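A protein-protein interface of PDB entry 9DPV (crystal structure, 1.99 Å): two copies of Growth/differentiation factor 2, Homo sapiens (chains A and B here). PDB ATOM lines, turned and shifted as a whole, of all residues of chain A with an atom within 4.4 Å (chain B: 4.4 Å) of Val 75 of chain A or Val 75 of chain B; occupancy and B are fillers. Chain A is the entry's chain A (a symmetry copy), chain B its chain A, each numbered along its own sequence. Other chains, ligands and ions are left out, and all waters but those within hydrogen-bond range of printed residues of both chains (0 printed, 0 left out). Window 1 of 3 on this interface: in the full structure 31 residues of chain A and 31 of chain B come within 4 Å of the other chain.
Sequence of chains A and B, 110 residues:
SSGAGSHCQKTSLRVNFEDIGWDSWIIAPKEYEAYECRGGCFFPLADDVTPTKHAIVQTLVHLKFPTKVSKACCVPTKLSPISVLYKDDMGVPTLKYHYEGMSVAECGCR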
ATOM      1  N   CYS A  37     -10.798 -15.578 -18.550  1.00  0.00           N
ATOM      2  CA  CYS A  37      -9.689 -16.517 -18.589  1.00  0.00           C
ATOM      3  C   CYS A  37      -9.866 -17.455 -19.775  1.00  0.00           C
ATOM      4  O   CYS A  37     -10.867 -18.161 -19.870  1.00  0.00           O
ATOM      5  CB  CYS A  37      -9.593 -17.274 -17.271  1.00  0.00           C
ATOM      6  SG  CYS A  37      -9.259 -16.208 -15.857  1.00  0.00           S
ATOM      7  N   CYS A  73      -9.891 -26.921 -16.537  1.00  0.00           N
ATOM      8  CA  CYS A  73     -10.449 -25.697 -17.080  1.00  0.00           C
ATOM      9  C   CYS A  73      -9.668 -24.457 -16.661  1.00  0.00           C
ATOM     10  O   CYS A  73      -9.280 -24.338 -15.503  1.00  0.00           O
ATOM     11  CB  CYS A  73     -11.900 -25.581 -16.653  1.00  0.00           C
ATOM     12  SG  CYS A  73     -12.953 -24.824 -17.903  1.00  0.00           S
ATOM     13  N   CYS A  74      -9.452 -23.556 -17.627  1.00  0.00           N
ATOM     14  CA  CYS A  74      -8.861 -22.250 -17.393  1.00  0.00           C
ATOM     15  C   CYS A  74      -9.908 -21.305 -16.812  1.00  0.00           C
ATOM     16  O   CYS A  74     -10.794 -20.850 -17.529  1.00  0.00           O
ATOM     17  CB  CYS A  74      -8.277 -21.695 -18.691  1.00  0.00           C
ATOM     18  SG  CYS A  74      -7.443 -20.101 -18.503  1.00  0.00           S
ATOM     19  N   VAL A  75      -9.788 -21.009 -15.516  1.00  0.00           N
ATOM     20  CA  VAL A  75     -10.777 -20.217 -14.803  1.00  0.00           C
ATOM     21  C   VAL A  75     -10.124 -19.097 -14.004  1.00  0.00           C
ATOM     22  O   VAL A  75      -8.922 -19.140 -13.729  1.00  0.00           O
ATOM     23  CB  VAL A  75     -11.601 -21.109 -13.837  1.00  0.00           C
ATOM     24  CG1 VAL A  75     -12.557 -22.024 -14.592  1.00  0.00           C
ATOM     25  CG2 VAL A  75     -10.685 -21.898 -12.908  1.00  0.00           C
ATOM     26  N   PRO A  76     -10.890 -18.060 -13.589  1.00  0.00           N
ATOM     27  CA  PRO A  76     -10.401 -17.115 -12.597  1.00  0.00           C
ATOM     28  C   PRO A  76     -10.076 -17.784 -11.268  1.00  0.00           C
ATOM     29  O   PRO A  76     -10.881 -18.559 -10.753  1.00  0.00           O
ATOM     30  CB  PRO A  76     -11.551 -16.107 -12.459  1.00  0.00           C
ATOM     31  CG  PRO A  76     -12.392 -16.308 -13.645  1.00  0.00           C
ATOM     32  CD  PRO A  76     -12.234 -17.730 -14.075  1.00  0.00           C
ATOM     33  N   THR A  77      -8.890 -17.478 -10.741  1.00  0.00           N
ATOM     34  CA  THR A  77      -8.455 -17.971  -9.448  1.00  0.00           C
ATOM     35  C   THR A  77      -8.366 -16.850  -8.415  1.00  0.00           C
ATOM     36  O   THR A  77      -8.128 -17.108  -7.240  1.00  0.00           O
ATOM     37  CB  THR A  77      -7.130 -18.690  -9.639  1.00  0.00           C
ATOM     38  OG1 THR A  77      -6.203 -17.776 -10.226  1.00  0.00           O
ATOM     39  CG2 THR A  77      -7.277 -19.904 -10.528  1.00  0.00           C
ATOM     40  N   GLU A 106      -6.484 -12.935 -11.611  1.00  0.00           N
ATOM     41  CA  GLU A 106      -5.599 -14.008 -12.041  1.00  0.00           C
ATOM     42  C   GLU A 106      -6.383 -15.204 -12.577  1.00  0.00           C
ATOM     43  O   GLU A 106      -7.487 -15.468 -12.123  1.00  0.00           O
ATOM     44  CB  GLU A 106      -4.716 -14.469 -10.862  1.00  0.00           C
ATOM     45  CG  GLU A 106      -3.471 -13.637 -10.659  1.00  0.00           C
ATOM     46  CD  GLU A 106      -2.957 -13.646  -9.237  1.00  0.00           C
ATOM     47  OE1 GLU A 106      -2.980 -14.727  -8.605  1.00  0.00           O
ATOM     48  OE2 GLU A 106      -2.524 -12.575  -8.755  1.00  0.00           O
ATOM     49  N   CYS A 107      -5.764 -15.926 -13.519  1.00  0.00           N
ATOM     50  CA  CYS A 107      -6.313 -17.124 -14.128  1.00  0.00           C
ATOM     51  C   CYS A 107      -5.451 -18.327 -13.755  1.00  0.00           C
ATOM     52  O   CYS A 107      -4.255 -18.190 -13.531  1.00  0.00           O
ATOM     53  CB  CYS A 107      -6.369 -16.985 -15.645  1.00  0.00           C
ATOM     54  SG  CYS A 107      -7.360 -15.599 -16.237  1.00  0.00           S
ATOM     55  N   GLY A 108      -6.057 -19.513 -13.739  1.00  0.00           N
ATOM     56  CA  GLY A 108      -5.293 -20.744 -13.623  1.00  0.00           C
ATOM     57  C   GLY A 108      -6.108 -21.957 -14.043  1.00  0.00           C
ATOM     58  O   GLY A 108      -7.310 -21.860 -14.263  1.00  0.00           O
ATOM     59  N   ARG A 110      -7.772 -25.491 -13.211  1.00  0.00           N
ATOM     60  CA  ARG A 110      -8.409 -26.074 -12.044  1.00  0.00           C
ATOM     61  C   ARG A 110      -9.240 -27.297 -12.442  1.00  0.00           C
ATOM     62  O   ARG A 110      -9.396 -28.232 -11.646  1.00  0.00           O
ATOM     63  CB  ARG A 110      -9.279 -25.026 -11.338  1.00  0.00           C
ATOM     64  CG  ARG A 110      -8.486 -23.892 -10.724  1.00  0.00           C
ATOM     65  CD  ARG A 110      -7.589 -24.378  -9.607  1.00  0.00           C
ATOM     66  NE  ARG A 110      -6.851 -23.294  -8.971  1.00  0.00           N
ATOM     67  CZ  ARG A 110      -5.671 -22.838  -9.369  1.00  0.00           C
ATOM     68  NH1 ARG A 110      -5.113 -23.237 -10.502  1.00  0.00           N
ATOM     69  NH2 ARG A 110      -5.037 -21.948  -8.614  1.00  0.00           N
ATOM     70  OXT ARG A 110      -9.739 -27.362 -13.563  1.00  0.00           O
ATOM     71  N   CYS B  37     -15.481 -32.691 -11.259  1.00  0.00           N
ATOM     72  CA  CYS B  37     -16.608 -31.773 -11.282  1.00  0.00           C
ATOM     73  C   CYS B  37     -17.194 -31.731 -12.687  1.00  0.00           C
ATOM     74  O   CYS B  37     -16.501 -31.387 -13.643  1.00  0.00           O
ATOM     75  CB  CYS B  37     -16.175 -30.394 -10.801  1.00  0.00           C
ATOM     76  SG  CYS B  37     -15.591 -30.382  -9.097  1.00  0.00           S
ATOM     77  N   CYS B  73     -17.188 -22.286 -15.992  1.00  0.00           N
ATOM     78  CA  CYS B  73     -16.768 -23.674 -15.920  1.00  0.00           C
ATOM     79  C   CYS B  73     -17.024 -24.297 -14.552  1.00  0.00           C
ATOM     80  O   CYS B  73     -16.772 -23.663 -13.532  1.00  0.00           O
ATOM     81  CB  CYS B  73     -15.297 -23.767 -16.280  1.00  0.00           C
ATOM     82  SG  CYS B  73     -14.878 -25.269 -17.183  1.00  0.00           S
ATOM     83  N   CYS B  74     -17.529 -25.537 -14.566  1.00  0.00           N
ATOM     84  CA  CYS B  74     -17.700 -26.350 -13.376  1.00  0.00           C
ATOM     85  C   CYS B  74     -16.360 -26.951 -12.963  1.00  0.00           C
ATOM     86  O   CYS B  74     -15.875 -27.877 -13.606  1.00  0.00           O
ATOM     87  CB  CYS B  74     -18.740 -27.441 -13.628  1.00  0.00           C
ATOM     88  SG  CYS B  74     -19.093 -28.471 -12.184  1.00  0.00           S
ATOM     89  N   VAL B  75     -15.781 -26.427 -11.881  1.00  0.00           N
ATOM     90  CA  VAL B  75     -14.454 -26.820 -11.440  1.00  0.00           C
ATOM     91  C   VAL B  75     -14.434 -27.150  -9.953  1.00  0.00           C
ATOM     92  O   VAL B  75     -15.336 -26.754  -9.211  1.00  0.00           O
ATOM     93  CB  VAL B  75     -13.426 -25.690 -11.718  1.00  0.00           C
ATOM     94  CG1 VAL B  75     -13.129 -25.549 -13.205  1.00  0.00           C
ATOM     95  CG2 VAL B  75     -13.891 -24.370 -11.111  1.00  0.00           C
ATOM     96  N   PRO B  76     -13.400 -27.872  -9.460  1.00  0.00           N
ATOM     97  CA  PRO B  76     -13.176 -27.980  -8.027  1.00  0.00           C
ATOM     98  C   PRO B  76     -12.918 -26.626  -7.377  1.00  0.00           C
ATOM     99  O   PRO B  76     -12.109 -25.846  -7.874  1.00  0.00           O
ATOM    100  CB  PRO B  76     -11.953 -28.903  -7.919  1.00  0.00           C
ATOM    101  CG  PRO B  76     -11.846 -29.562  -9.226  1.00  0.00           C
ATOM    102  CD  PRO B  76     -12.430 -28.643 -10.247  1.00  0.00           C
ATOM    103  N   THR B  77     -13.626 -26.371  -6.275  1.00  0.00           N
ATOM    104  CA  THR B  77     -13.450 -25.161  -5.494  1.00  0.00           C
ATOM    105  C   THR B  77     -12.834 -25.453  -4.128  1.00  0.00           C
ATOM    106  O   THR B  77     -12.507 -24.532  -3.386  1.00  0.00           O
ATOM    107  CB  THR B  77     -14.800 -24.470  -5.385  1.00  0.00           C
ATOM    108  OG1 THR B  77     -15.726 -25.383  -4.796  1.00  0.00           O
ATOM    109  CG2 THR B  77     -15.312 -24.031  -6.738  1.00  0.00           C
ATOM    110  N   GLU B 106     -15.345 -30.107  -3.071  1.00  0.00           N
ATOM    111  CA  GLU B 106     -16.494 -29.343  -3.537  1.00  0.00           C
ATOM    112  C   GLU B 106     -16.286 -28.824  -4.958  1.00  0.00           C
ATOM    113  O   GLU B 106     -15.162 -28.537  -5.349  1.00  0.00           O
ATOM    114  CB  GLU B 106     -16.752 -28.149  -2.594  1.00  0.00           C
ATOM    115  CG  GLU B 106     -17.579 -28.490  -1.376  1.00  0.00           C
ATOM    116  CD  GLU B 106     -17.327 -27.581  -0.195  1.00  0.00           C
ATOM    117  OE1 GLU B 106     -17.181 -26.356  -0.409  1.00  0.00           O
ATOM    118  OE2 GLU B 106     -17.282 -28.092   0.948  1.00  0.00           O
ATOM    119  N   CYS B 107     -17.397 -28.680  -5.690  1.00  0.00           N
ATOM    120  CA  CYS B 107     -17.426 -28.160  -7.045  1.00  0.00           C
ATOM    121  C   CYS B 107     -18.185 -26.836  -7.068  1.00  0.00           C
ATOM    122  O   CYS B 107     -19.077 -26.617  -6.259  1.00  0.00           O
ATOM    123  CB  CYS B 107     -18.094 -29.151  -7.992  1.00  0.00           C
ATOM    124  SG  CYS B 107     -17.301 -30.769  -8.072  1.00  0.00           S
ATOM    125  N   GLY B 108     -17.858 -25.978  -8.033  1.00  0.00           N
ATOM    126  CA  GLY B 108     -18.662 -24.796  -8.290  1.00  0.00           C
ATOM    127  C   GLY B 108     -18.374 -24.201  -9.659  1.00  0.00           C
ATOM    128  O   GLY B 108     -17.436 -24.608 -10.335  1.00  0.00           O
ATOM    129  N   ARG B 110     -17.139 -21.171 -11.948  1.00  0.00           N
ATOM    130  CA  ARG B 110     -16.122 -20.141 -11.825  1.00  0.00           C
ATOM    131  C   ARG B 110     -15.811 -19.529 -13.193  1.00  0.00           C
ATOM    132  O   ARG B 110     -15.446 -18.350 -13.281  1.00  0.00           O
ATOM    133  CB  ARG B 110     -14.856 -20.725 -11.184  1.00  0.00           C
ATOM    134  CG  ARG B 110     -15.045 -21.148  -9.742  1.00  0.00           C
ATOM    135  CD  ARG B 110     -15.350 -19.968  -8.848  1.00  0.00           C
ATOM    136  NE  ARG B 110     -15.488 -20.347  -7.448  1.00  0.00           N
ATOM    137  CZ  ARG B 110     -16.617 -20.743  -6.873  1.00  0.00           C
ATOM    138  NH1 ARG B 110     -17.714 -20.978  -7.576  1.00  0.00           N
ATOM    139  NH2 ARG B 110     -16.641 -20.916  -5.557  1.00  0.00           N
ATOM    140  OXT ARG B 110     -15.942 -20.204 -14.212  1.00  0.00           O
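The side-chain sulfur (SG) of Cys 73 of chain B is disulfide-bonded to the side-chain sulfur (SG) of Cys 73 of chain A, at 2.1 Å.
The backbone carbonyl oxygen (O) of Cys 73 of chain B lies within hydrogen-bond range of the backbone NH (N) of Arg 110 of chain B (3.0 Å). O of Val 75 of chain B sits at hydrogen-bond distance from N of Gly 108 of chain B (2.9 Å). The backbone carbonyl oxygen (O) of Cys 73 of chain A lies within hydrogen-bond range of the backbone NH (N) of Arg 110 of chain A, 3.0 Å away. The backbone NH (N) of Gly 108 of chain A lies within hydrogen-bond range of the backbone carbonyl oxygen (O) of Val 75 of chain A (2.9 Å). The side-chain sulfur (SG) of Cys 107 of chain B is disulfide-bonded to the side-chain sulfur (SG) of Cys 37 of chain B (2.0 Å). SG of Cys 37 of chain A is disulfide-bonded to SG of Cys 107 of chain A (2.0 Å).
Val 75 of chain B touches Cys 73 of chain A. Cys 73 of chain B touches Val 75 of chain A (CB to CG1, 3.7 Å). CG1 of Val 75 of chain A touches CG1 of Val 75 of chain B (3.8 Å). Arg 110 of chain B touches Val 75 of chain A (OXT to CG1, 3.9 Å). Arg 110 of chain B touches Pro 76 of chain A. CG1 of Val 75 of chain B touches OXT of Arg 110 of chain A, at 3.9 Å. O of Arg 110 of chain A touches CD of Pro 76 of chain B, 3.4 Å away.
Printed residues of chain B within 4 Å of Cys 73 of chain A: Cys 73 (2.1 Å) and Val 75 (3.7 Å). Of chain B, only Cys 73, Val 75 and Arg 110 come within 4 Å of Val 75 of chain A. Gly 108 of chain A touches none of the printed residues of chain B. Of the printed residues of chain B, Arg 110 of chain A touches Val 75 (3.9 Å) and Pro 76 (3.4 Å). Of the printed residues of chain A, Cys 73 of chain B touches Cys 73 and Val 75. Printed residues of chain A within 4 Å of Pro 76 of chain B: Arg 110 (3.4 Å). Glu 106 of chain B touches none of the printed residues of chain A. Printed residues of chain A within 4 Å of Arg 110 of chain B: Val 75 (3.9 Å) and Pro 76 (3.4 Å). The nearest printed residue of chain B that does not touch Val 75 of chain A is Cys 74 of chain B (6.1 Å). The nearest printed residue of chain A that does not touch Pro 76 of chain B is Val 75 of chain A (6.6 Å).
Printed residues of chain B that touch a printed residue of chain A: Cys 73, Val 75, Pro 76 and Arg 110. Hydrophobic or aromatic side chains of chain B that line the printed part of chain A: Val 75 and Pro 76. Of the 10 printed residues of chain A, 4 touch a printed residue of chain B. Hydrophobic or aromatic side chains of chain A that line the printed part of chain B: Val 75 and Pro 76. Among the printed residues, 8 pairs touch across the chains.
Cys 73 of chain B touches its own counterpart, Cys 73 of chain A. Cys 73 of chain A touches Val 75 of chain B, and with the chains exchanged Val 75 of chain A touches Cys 73 of chain B. Val 75 of chain A touches its own counterpart, Val 75 of chain B. Val 75 of chain A touches Arg 110 of chain B, and with the chains exchanged Arg 110 of chain A touches Val 75 of chain B.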
